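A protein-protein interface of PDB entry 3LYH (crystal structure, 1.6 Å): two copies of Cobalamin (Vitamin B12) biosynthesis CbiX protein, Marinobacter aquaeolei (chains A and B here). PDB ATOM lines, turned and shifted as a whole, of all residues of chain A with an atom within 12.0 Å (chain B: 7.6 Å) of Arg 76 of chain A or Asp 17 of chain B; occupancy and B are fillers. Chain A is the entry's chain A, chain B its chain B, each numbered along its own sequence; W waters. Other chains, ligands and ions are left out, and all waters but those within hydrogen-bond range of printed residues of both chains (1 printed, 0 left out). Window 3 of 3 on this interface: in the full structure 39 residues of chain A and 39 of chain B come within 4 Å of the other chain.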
ATOM      1  N   HIS A  13     -29.747  19.197 -16.773  1.00  0.00           N
ATOM      2  CA  HIS A  13     -29.540  20.501 -16.188  1.00  0.00           C
ATOM      3  C   HIS A  13     -30.353  20.525 -14.911  1.00  0.00           C
ATOM      4  O   HIS A  13     -31.528  20.162 -14.881  1.00  0.00           O
ATOM      5  CB  HIS A  13     -29.966  21.630 -17.119  1.00  0.00           C
ATOM      6  CG  HIS A  13     -28.813  22.301 -17.796  1.00  0.00           C
ATOM      7  ND1 HIS A  13     -27.657  22.636 -17.124  1.00  0.00           N
ATOM      8  CD2 HIS A  13     -28.629  22.684 -19.080  1.00  0.00           C
ATOM      9  CE1 HIS A  13     -26.811  23.203 -17.966  1.00  0.00           C
ATOM     10  NE2 HIS A  13     -27.377  23.241 -19.160  1.00  0.00           N
ATOM     11  N   MET A  43     -26.155  18.529 -13.511  1.00  0.00           N
ATOM     12  CA  MET A  43     -24.916  19.265 -13.771  1.00  0.00           C
ATOM     13  C   MET A  43     -24.655  20.286 -12.722  1.00  0.00           C
ATOM     14  O   MET A  43     -23.500  20.517 -12.385  1.00  0.00           O
ATOM     15  CB  MET A  43     -24.887  19.956 -15.133  1.00  0.00           C
ATOM     16  CG  MET A  43     -24.681  18.994 -16.233  1.00  0.00           C
ATOM     17  SD  MET A  43     -24.636  20.007 -17.875  1.00  0.00           S
ATOM     18  CE  MET A  43     -22.908  20.823 -17.926  1.00  0.00           C
ATOM     19  N   PHE A  71     -31.138  16.299 -22.714  1.00  0.00           N
ATOM     20  CA  PHE A  71     -31.159  17.614 -23.370  1.00  0.00           C
ATOM     21  C   PHE A  71     -31.856  17.401 -24.696  1.00  0.00           C
ATOM     22  O   PHE A  71     -31.489  16.473 -25.439  1.00  0.00           O
ATOM     23  CB  PHE A  71     -29.764  18.151 -23.792  1.00  0.00           C
ATOM     24  CG  PHE A  71     -28.724  18.236 -22.700  1.00  0.00           C
ATOM     25  CD1 PHE A  71     -29.052  18.436 -21.374  1.00  0.00           C
ATOM     26  CD2 PHE A  71     -27.377  18.123 -23.046  1.00  0.00           C
ATOM     27  CE1 PHE A  71     -28.047  18.521 -20.403  1.00  0.00           C
ATOM     28  CE2 PHE A  71     -26.396  18.203 -22.099  1.00  0.00           C
ATOM     29  CZ  PHE A  71     -26.716  18.404 -20.786  1.00  0.00           C
ATOM     30  N   LEU A  72     -32.809  18.269 -25.043  1.00  0.00           N
ATOM     31  CA  LEU A  72     -33.323  18.270 -26.409  1.00  0.00           C
ATOM     32  C   LEU A  72     -32.295  18.751 -27.422  1.00  0.00           C
ATOM     33  O   LEU A  72     -32.331  18.317 -28.556  1.00  0.00           O
ATOM     34  CB  LEU A  72     -34.632  19.049 -26.541  1.00  0.00           C
ATOM     35  CG  LEU A  72     -35.809  18.491 -25.713  1.00  0.00           C
ATOM     36  CD1 LEU A  72     -37.053  19.375 -25.757  1.00  0.00           C
ATOM     37  CD2 LEU A  72     -36.155  17.100 -26.233  1.00  0.00           C
ATOM     38  N   ALA A  73     -31.435  19.687 -27.020  1.00  0.00           N
ATOM     39  CA  ALA A  73     -30.317  20.097 -27.855  1.00  0.00           C
ATOM     40  C   ALA A  73     -29.187  20.646 -27.013  1.00  0.00           C
ATOM     41  O   ALA A  73     -29.405  21.085 -25.886  1.00  0.00           O
ATOM     42  CB  ALA A  73     -30.762  21.143 -28.850  1.00  0.00           C
ATOM     43  N   ALA A  74     -28.008  20.705 -27.623  1.00  0.00           N
ATOM     44  CA  ALA A  74     -26.824  21.279 -26.950  1.00  0.00           C
ATOM     45  C   ALA A  74     -26.289  22.398 -27.803  1.00  0.00           C
ATOM     46  O   ALA A  74     -25.837  22.155 -28.931  1.00  0.00           O
ATOM     47  CB  ALA A  74     -25.762  20.245 -26.782  1.00  0.00           C
ATOM     48  N   GLY A  75     -26.278  23.609 -27.252  1.00  0.00           N
ATOM     49  CA  GLY A  75     -25.587  24.751 -27.876  1.00  0.00           C
ATOM     50  C   GLY A  75     -24.074  24.716 -27.756  1.00  0.00           C
ATOM     51  O   GLY A  75     -23.507  23.755 -27.225  1.00  0.00           O
ATOM     52  N   ARG A  76     -23.394  25.770 -28.234  1.00  0.00           N
ATOM     53  CA  ARG A  76     -21.917  25.810 -28.217  1.00  0.00           C
ATOM     54  C   ARG A  76     -21.261  25.590 -26.861  1.00  0.00           C
ATOM     55  O   ARG A  76     -20.305  24.815 -26.760  1.00  0.00           O
ATOM     56  CB  ARG A  76     -21.371  27.134 -28.785  1.00  0.00           C
ATOM     57  CG  ARG A  76     -19.841  27.168 -28.878  1.00  0.00           C
ATOM     58  N   HIS A  77     -21.778  26.249 -25.827  1.00  0.00           N
ATOM     59  CA  HIS A  77     -21.249  26.041 -24.461  1.00  0.00           C
ATOM     60  C   HIS A  77     -21.389  24.579 -23.975  1.00  0.00           C
ATOM     61  O   HIS A  77     -20.369  23.972 -23.619  1.00  0.00           O
ATOM     62  CB  HIS A  77     -21.847  27.043 -23.457  1.00  0.00           C
ATOM     63  CG  HIS A  77     -21.366  28.449 -23.674  1.00  0.00           C
ATOM     64  ND1 HIS A  77     -20.031  28.761 -23.825  1.00  0.00           N
ATOM     65  CD2 HIS A  77     -22.042  29.618 -23.798  1.00  0.00           C
ATOM     66  CE1 HIS A  77     -19.902  30.061 -24.026  1.00  0.00           C
ATOM     67  NE2 HIS A  77     -21.108  30.605 -24.014  1.00  0.00           N
ATOM     68  N   LEU A  78     -22.594  24.001 -24.036  1.00  0.00           N
ATOM     69  CA  LEU A  78     -22.796  22.585 -23.628  1.00  0.00           C
ATOM     70  C   LEU A  78     -21.882  21.662 -24.388  1.00  0.00           C
ATOM     71  O   LEU A  78     -21.361  20.716 -23.836  1.00  0.00           O
ATOM     72  CB  LEU A  78     -24.243  22.084 -23.812  1.00  0.00           C
ATOM     73  CG  LEU A  78     -25.248  22.313 -22.695  1.00  0.00           C
ATOM     74  CD1 LEU A  78     -26.599  21.804 -23.070  1.00  0.00           C
ATOM     75  CD2 LEU A  78     -24.790  21.709 -21.331  1.00  0.00           C
ATOM     76  N   ARG A  79     -21.708  21.902 -25.682  1.00  0.00           N
ATOM     77  CA  ARG A  79     -20.831  21.041 -26.524  1.00  0.00           C
ATOM     78  C   ARG A  79     -19.370  20.961 -26.088  1.00  0.00           C
ATOM     79  O   ARG A  79     -18.725  19.961 -26.298  1.00  0.00           O
ATOM     80  CB  ARG A  79     -20.898  21.479 -27.980  1.00  0.00           C
ATOM     81  CG  ARG A  79     -22.194  21.115 -28.637  1.00  0.00           C
ATOM     82  CD  ARG A  79     -22.173  21.337 -30.140  1.00  0.00           C
ATOM     83  NE  ARG A  79     -21.781  22.661 -30.652  1.00  0.00           N
ATOM     84  CZ  ARG A  79     -22.640  23.638 -31.009  1.00  0.00           C
ATOM     85  NH1 ARG A  79     -23.953  23.518 -30.814  1.00  0.00           N
ATOM     86  NH2 ARG A  79     -22.169  24.778 -31.524  1.00  0.00           N
ATOM     87  N   LYS A  80     -18.876  22.040 -25.497  1.00  0.00           N
ATOM     88  CA  LYS A  80     -17.524  22.106 -24.966  1.00  0.00           C
ATOM     89  C   LYS A  80     -17.542  21.623 -23.526  1.00  0.00           C
ATOM     90  O   LYS A  80     -16.688  20.833 -23.120  1.00  0.00           O
ATOM     91  CB  LYS A  80     -17.011  23.547 -25.032  1.00  0.00           C
ATOM     92  CG  LYS A  80     -15.562  23.710 -24.526  1.00  0.00           C
ATOM     93  CD  LYS A  80     -15.257  25.177 -24.252  1.00  0.00           C
ATOM     94  CE  LYS A  80     -13.954  25.332 -23.489  1.00  0.00           C
ATOM     95  NZ  LYS A  80     -12.837  25.046 -24.395  1.00  0.00           N
ATOM     96  N   ASP A  81     -18.533  22.062 -22.762  1.00  0.00           N
ATOM     97  CA  ASP A  81     -18.450  21.914 -21.310  1.00  0.00           C
ATOM     98  C   ASP A  81     -18.788  20.520 -20.811  1.00  0.00           C
ATOM     99  O   ASP A  81     -18.291  20.088 -19.759  1.00  0.00           O
ATOM    100  CB  ASP A  81     -19.393  22.888 -20.608  1.00  0.00           C
ATOM    101  CG  ASP A  81     -18.990  24.361 -20.787  1.00  0.00           C
ATOM    102  OD1 ASP A  81     -17.869  24.675 -21.261  1.00  0.00           O
ATOM    103  OD2 ASP A  81     -19.851  25.198 -20.460  1.00  0.00           O
ATOM    104  N   VAL A  82     -19.729  19.844 -21.474  1.00  0.00           N
ATOM    105  CA  VAL A  82     -20.107  18.513 -20.994  1.00  0.00           C
ATOM    106  C   VAL A  82     -18.938  17.533 -21.209  1.00  0.00           C
ATOM    107  O   VAL A  82     -18.571  16.831 -20.293  1.00  0.00           O
ATOM    108  CB  VAL A  82     -21.452  18.001 -21.591  1.00  0.00           C
ATOM    109  CG1 VAL A  82     -21.740  16.568 -21.146  1.00  0.00           C
ATOM    110  CG2 VAL A  82     -22.561  18.925 -21.138  1.00  0.00           C
ATOM    111  N   PRO A  83     -18.353  17.466 -22.420  1.00  0.00           N
ATOM    112  CA  PRO A  83     -17.185  16.584 -22.525  1.00  0.00           C
ATOM    113  C   PRO A  83     -16.021  16.952 -21.621  1.00  0.00           C
ATOM    114  O   PRO A  83     -15.359  16.056 -21.154  1.00  0.00           O
ATOM    115  CB  PRO A  83     -16.761  16.714 -23.989  1.00  0.00           C
ATOM    116  CG  PRO A  83     -18.017  17.054 -24.698  1.00  0.00           C
ATOM    117  CD  PRO A  83     -18.753  17.983 -23.739  1.00  0.00           C
ATOM    118  N   ALA A  84     -15.816  18.245 -21.343  1.00  0.00           N
ATOM    119  CA  ALA A  84     -14.751  18.646 -20.389  1.00  0.00           C
ATOM    120  C   ALA A  84     -15.057  18.122 -18.998  1.00  0.00           C
ATOM    121  O   ALA A  84     -14.157  17.616 -18.292  1.00  0.00           O
ATOM    122  CB  ALA A  84     -14.572  20.164 -20.352  1.00  0.00           C
ATOM    123  N   MET A  85     -16.333  18.194 -18.620  1.00  0.00           N
ATOM    124  CA  MET A  85     -16.790  17.667 -17.330  1.00  0.00           C
ATOM    125  C   MET A  85     -16.554  16.145 -17.270  1.00  0.00           C
ATOM    126  O   MET A  85     -16.081  15.646 -16.227  1.00  0.00           O
ATOM    127  CB  MET A  85     -18.267  18.052 -17.034  1.00  0.00           C
ATOM    128  CG  MET A  85     -18.782  17.579 -15.706  1.00  0.00           C
ATOM    129  SD  MET A  85     -20.691  17.872 -15.609  1.00  0.00           S
ATOM    130  CE  MET A  85     -20.655  19.725 -14.987  1.00  0.00           C
ATOM    131  N   LEU A  99     -19.736   9.282 -23.199  1.00  0.00           N
ATOM    132  CA  LEU A  99     -20.762  10.278 -23.360  1.00  0.00           C
ATOM    133  C   LEU A  99     -21.600   9.949 -24.607  1.00  0.00           C
ATOM    134  O   LEU A  99     -21.136  10.015 -25.759  1.00  0.00           O
ATOM    135  CB  LEU A  99     -20.153  11.667 -23.459  1.00  0.00           C
ATOM    136  CG  LEU A  99     -21.092  12.840 -23.593  1.00  0.00           C
ATOM    137  CD1 LEU A  99     -22.018  12.928 -22.364  1.00  0.00           C
ATOM    138  CD2 LEU A  99     -20.276  14.117 -23.776  1.00  0.00           C
ATOM    139  N   PRO A 102     -27.019  13.581 -26.986  1.00  0.00           N
ATOM    140  CA  PRO A 102     -28.242  14.037 -26.273  1.00  0.00           C
ATOM    141  C   PRO A 102     -29.501  13.357 -26.815  1.00  0.00           C
ATOM    142  O   PRO A 102     -29.545  12.997 -27.974  1.00  0.00           O
ATOM    143  CB  PRO A 102     -28.279  15.539 -26.533  1.00  0.00           C
ATOM    144  CG  PRO A 102     -27.290  15.817 -27.631  1.00  0.00           C
ATOM    145  CD  PRO A 102     -26.372  14.662 -27.771  1.00  0.00           C
ATOM    146  N   LYS A 105     -31.217  14.204 -30.183  1.00  0.00           N
ATOM    147  CA  LYS A 105     -30.724  13.728 -31.470  1.00  0.00           C
ATOM    148  C   LYS A 105     -31.329  12.413 -31.910  1.00  0.00           C
ATOM    149  O   LYS A 105     -31.141  12.009 -33.063  1.00  0.00           O
ATOM    150  CB  LYS A 105     -29.169  13.634 -31.486  1.00  0.00           C
ATOM    151  CG  LYS A 105     -28.483  15.004 -31.510  1.00  0.00           C
ATOM    152  CD  LYS A 105     -26.988  14.818 -31.924  1.00  0.00           C
ATOM    153  CE  LYS A 105     -26.296  16.128 -32.327  1.00  0.00           C
ATOM    154  NZ  LYS A 105     -24.962  15.886 -33.009  1.00  0.00           N
ATOM    155  N   GLY B  14     -35.119  29.840 -29.703  1.00  0.00           N
ATOM    156  CA  GLY B  14     -34.221  30.003 -30.845  1.00  0.00           C
ATOM    157  C   GLY B  14     -32.809  30.329 -30.395  1.00  0.00           C
ATOM    158  O   GLY B  14     -32.528  30.490 -29.214  1.00  0.00           O
ATOM    159  N   SER B  15     -31.937  30.473 -31.370  1.00  0.00           N
ATOM    160  CA  SER B  15     -30.540  30.692 -31.103  1.00  0.00           C
ATOM    161  C   SER B  15     -29.971  31.087 -32.419  1.00  0.00           C
ATOM    162  O   SER B  15     -30.522  30.742 -33.478  1.00  0.00           O
ATOM    163  CB  SER B  15     -29.897  29.404 -30.575  1.00  0.00           C
ATOM    164  OG  SER B  15     -28.510  29.603 -30.310  1.00  0.00           O
ATOM    165  N   SER B  16     -28.871  31.819 -32.374  1.00  0.00           N
ATOM    166  CA  SER B  16     -28.043  31.972 -33.550  1.00  0.00           C
ATOM    167  C   SER B  16     -27.217  30.699 -33.811  1.00  0.00           C
ATOM    168  O   SER B  16     -26.636  30.575 -34.880  1.00  0.00           O
ATOM    169  CB  SER B  16     -27.124  33.192 -33.413  1.00  0.00           C
ATOM    170  OG  SER B  16     -26.299  33.028 -32.279  1.00  0.00           O
ATOM    171  N   ASP B  17     -27.171  29.749 -32.862  1.00  0.00           N
ATOM    172  CA  ASP B  17     -26.394  28.519 -33.041  1.00  0.00           C
ATOM    173  C   ASP B  17     -27.106  27.603 -34.029  1.00  0.00           C
ATOM    174  O   ASP B  17     -28.234  27.191 -33.806  1.00  0.00           O
ATOM    175  CB  ASP B  17     -26.166  27.817 -31.700  1.00  0.00           C
ATOM    176  CG  ASP B  17     -25.232  26.632 -31.818  1.00  0.00           C
ATOM    177  OD1 ASP B  17     -24.004  26.862 -32.023  1.00  0.00           O
ATOM    178  OD2 ASP B  17     -25.706  25.482 -31.728  1.00  0.00           O
ATOM    179  N   ALA B  18     -26.443  27.327 -35.134  1.00  0.00           N
ATOM    180  CA  ALA B  18     -27.005  26.514 -36.216  1.00  0.00           C
ATOM    181  C   ALA B  18     -27.373  25.111 -35.784  1.00  0.00           C
ATOM    182  O   ALA B  18     -28.445  24.618 -36.108  1.00  0.00           O
ATOM    183  CB  ALA B  18     -25.976  26.463 -37.381  1.00  0.00           C
ATOM    184  N   ARG B  19     -26.477  24.472 -35.032  1.00  0.00           N
ATOM    185  CA  ARG B  19     -26.691  23.135 -34.535  1.00  0.00           C
ATOM    186  C   ARG B  19     -27.925  23.041 -33.609  1.00  0.00           C
ATOM    187  O   ARG B  19     -28.686  22.094 -33.698  1.00  0.00           O
ATOM    188  CB  ARG B  19     -25.446  22.617 -33.800  1.00  0.00           C
ATOM    189  CG  ARG B  19     -25.476  21.130 -33.497  1.00  0.00           C
ATOM    190  N   TRP B  20     -28.106  24.031 -32.728  1.00  0.00           N
ATOM    191  CA  TRP B  20     -29.239  24.101 -31.865  1.00  0.00           C
ATOM    192  C   TRP B  20     -30.543  24.079 -32.696  1.00  0.00           C
ATOM    193  O   TRP B  20     -31.443  23.258 -32.439  1.00  0.00           O
ATOM    194  CB  TRP B  20     -29.138  25.389 -31.056  1.00  0.00           C
ATOM    195  CG  TRP B  20     -30.306  25.685 -30.238  1.00  0.00           C
ATOM    196  CD1 TRP B  20     -31.469  26.342 -30.640  1.00  0.00           C
ATOM    197  CD2 TRP B  20     -30.480  25.349 -28.873  1.00  0.00           C
ATOM    198  NE1 TRP B  20     -32.335  26.421 -29.586  1.00  0.00           N
ATOM    199  CE2 TRP B  20     -31.741  25.856 -28.479  1.00  0.00           C
ATOM    200  CE3 TRP B  20     -29.678  24.686 -27.921  1.00  0.00           C
ATOM    201  CZ2 TRP B  20     -32.241  25.685 -27.177  1.00  0.00           C
ATOM    202  CZ3 TRP B  20     -30.158  24.540 -26.633  1.00  0.00           C
ATOM    203  CH2 TRP B  20     -31.437  25.027 -26.271  1.00  0.00           C
ATOM    204  N   CYS B  21     -30.650  25.030 -33.629  1.00  0.00           N
ATOM    205  CA  CYS B  21     -31.871  25.156 -34.445  1.00  0.00           C
ATOM    206  C   CYS B  21     -32.128  23.891 -35.285  1.00  0.00           C
ATOM    207  O   CYS B  21     -33.285  23.401 -35.319  1.00  0.00           O
ATOM    208  CB  CYS B  21     -31.827  26.386 -35.328  1.00  0.00           C
ATOM    209  SG  CYS B  21     -31.838  27.921 -34.349  1.00  0.00           S
ATOM    210  N   GLU B  22     -31.078  23.351 -35.895  1.00  0.00           N
ATOM    211  CA  GLU B  22     -31.135  22.076 -36.680  1.00  0.00           C
ATOM    212  C   GLU B  22     -31.698  20.932 -35.836  1.00  0.00           C
ATOM    213  O   GLU B  22     -32.463  20.096 -36.318  1.00  0.00           O
ATOM    214  CB  GLU B  22     -29.733  21.704 -37.230  1.00  0.00           C
ATOM    215  CG  GLU B  22     -29.574  20.293 -37.891  1.00  0.00           C
ATOM    216  CD  GLU B  22     -28.238  19.599 -37.537  1.00  0.00           C
ATOM    217  OE1 GLU B  22     -27.158  20.230 -37.651  1.00  0.00           O
ATOM    218  OE2 GLU B  22     -28.273  18.411 -37.147  1.00  0.00           O
ATOM    219  N   THR B  23     -31.259  20.843 -34.594  1.00  0.00           N
ATOM    220  CA  THR B  23     -31.775  19.783 -33.701  1.00  0.00           C
ATOM    221  C   THR B  23     -33.268  19.942 -33.504  1.00  0.00           C
ATOM    222  O   THR B  23     -34.030  18.952 -33.548  1.00  0.00           O
ATOM    223  CB  THR B  23     -30.975  19.758 -32.386  1.00  0.00           C
ATOM    224  OG1 THR B  23     -29.574  19.724 -32.698  1.00  0.00           O
ATOM    225  CG2 THR B  23     -31.370  18.519 -31.551  1.00  0.00           C
ATOM    226  N   LEU B  45     -34.768  34.999 -31.491  1.00  0.00           N
ATOM    227  CA  LEU B  45     -33.442  34.815 -32.128  1.00  0.00           C
ATOM    228  C   LEU B  45     -33.358  34.020 -33.449  1.00  0.00           C
ATOM    229  O   LEU B  45     -32.299  34.006 -34.102  1.00  0.00           O
ATOM    230  CB  LEU B  45     -32.436  34.236 -31.138  1.00  0.00           C
ATOM    231  CG  LEU B  45     -32.233  35.014 -29.839  1.00  0.00           C
ATOM    232  CD1 LEU B  45     -31.430  34.159 -28.845  1.00  0.00           C
ATOM    233  CD2 LEU B  45     -31.573  36.349 -30.076  1.00  0.00           C
ATOM    234  N   ALA B  46     -34.427  33.335 -33.837  1.00  0.00           N
ATOM    235  CA  ALA B  46     -34.447  32.575 -35.082  1.00  0.00           C
ATOM    236  C   ALA B  46     -35.809  32.729 -35.733  1.00  0.00           C
ATOM    237  O   ALA B  46     -36.793  32.995 -35.041  1.00  0.00           O
ATOM    238  CB  ALA B  46     -34.123  31.082 -34.826  1.00  0.00           C
HETATM  239  O   HOH W   1     -27.914  19.279 -30.280  1.00  0.00           O
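Printed residues of chain B within 4 Å of Leu 72 of chain A: Thr 23.
Of the printed residues of chain B, Ala 73 of chain A touches Trp 20 (3.6 Å) and Thr 23 (3.8 Å).
Of the printed residues of chain B, Gly 75 of chain A touches Asp 17 (3.9 Å) and Trp 20 (3.6 Å).
Printed residues of chain B within 4 Å of Arg 76 of chain A: Asp 17.
Printed residues of chain B within 4 Å of Arg 79 of chain A: Asp 17 and Arg 19.
No residue of chain A comes within 4 Å of Ser 16 of chain B.
Of the printed residues of chain A, Asp 17 of chain B touches Gly 75 (3.9 Å), Arg 76 (3.99 Å) and Arg 79 (2.8 Å).
No residue of chain A comes within 4 Å of Ala 18 of chain B.
Of chain A, only Arg 79 (3.5 Å) comes within 4 Å of Arg 19 of chain B.
No residue of chain A comes within 4 Å of Cys 21 of chain B.
Printed residues of chain A within 4 Å of Thr 23 of chain B: Leu 72 (3.2 Å) and Ala 73 (3.8 Å).
The nearest printed residue of chain A that does not touch Asp 17 of chain B is Ala 74 of chain A (4.3 Å).
Among the printed residues, merely in contact across the chains: Leu 72 of chain A with Thr 23 of chain B (3.2 Å), Arg 79 of chain A with Arg 19 of chain B (3.5 Å), Ala 73 of chain A with Trp 20 of chain B (3.6 Å), Gly 75 of chain A with Trp 20 of chain B (3.6 Å), Ala 73 of chain A with Thr 23 of chain B (3.8 Å), Gly 75 of chain A with Asp 17 of chain B (3.9 Å) and Arg 76 of chain A with Asp 17 of chain B (3.99 Å).
NH1 of Arg 79 of chain A lies within salt-bridge range of OD2 of Asp 17 of chain B, 2.8 Å away.
Water W1 bridges the side-chain hydroxyl (OG1) of Thr 23 of chain B (3.0 Å) and the backbone NH (N) of Ala 74 of chain A (3.0 Å).
O of Ala 74 of chain A lies within hydrogen-bond range of NH1 of Arg 79 of chain A, 3.0 Å away.
OG of Ser 15 of chain B is in hydrogen-bond range of N of Asp 17 of chain B, at 2.9 Å.
OD2 of Asp 17 of chain B is in hydrogen-bond range of N of Trp 20 of chain B, at 3.0 Å.
The side-chain sulfur of Cys 21 of chain B sits at hydrogen-bond distance from the backbone carbonyl oxygen of Asp 17 of chain B, 3.7 Å away.
The backbone carbonyl oxygen (O) of Arg 19 of chain B lies within hydrogen-bond range of the side-chain hydroxyl (OG1) of Thr 23 of chain B (2.7 Å).
No position is printed for both chains.
Of the 8 pairs that touch across the chains among the printed residues, none has its exchanged pair printed and touching as well.
Of the 20 printed residues of chain A, 5 touch a printed residue of chain B.
Hydrophobic or aromatic side chains of chain A within 4 Å of the printed part of chain B: Ala 73.
Printed residues of chain B that touch a printed residue of chain A: Asp 17, Arg 19, Trp 20 and Thr 23.
Hydrophobic or aromatic side chains of chain B that line the printed part of chain A: Trp 20.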
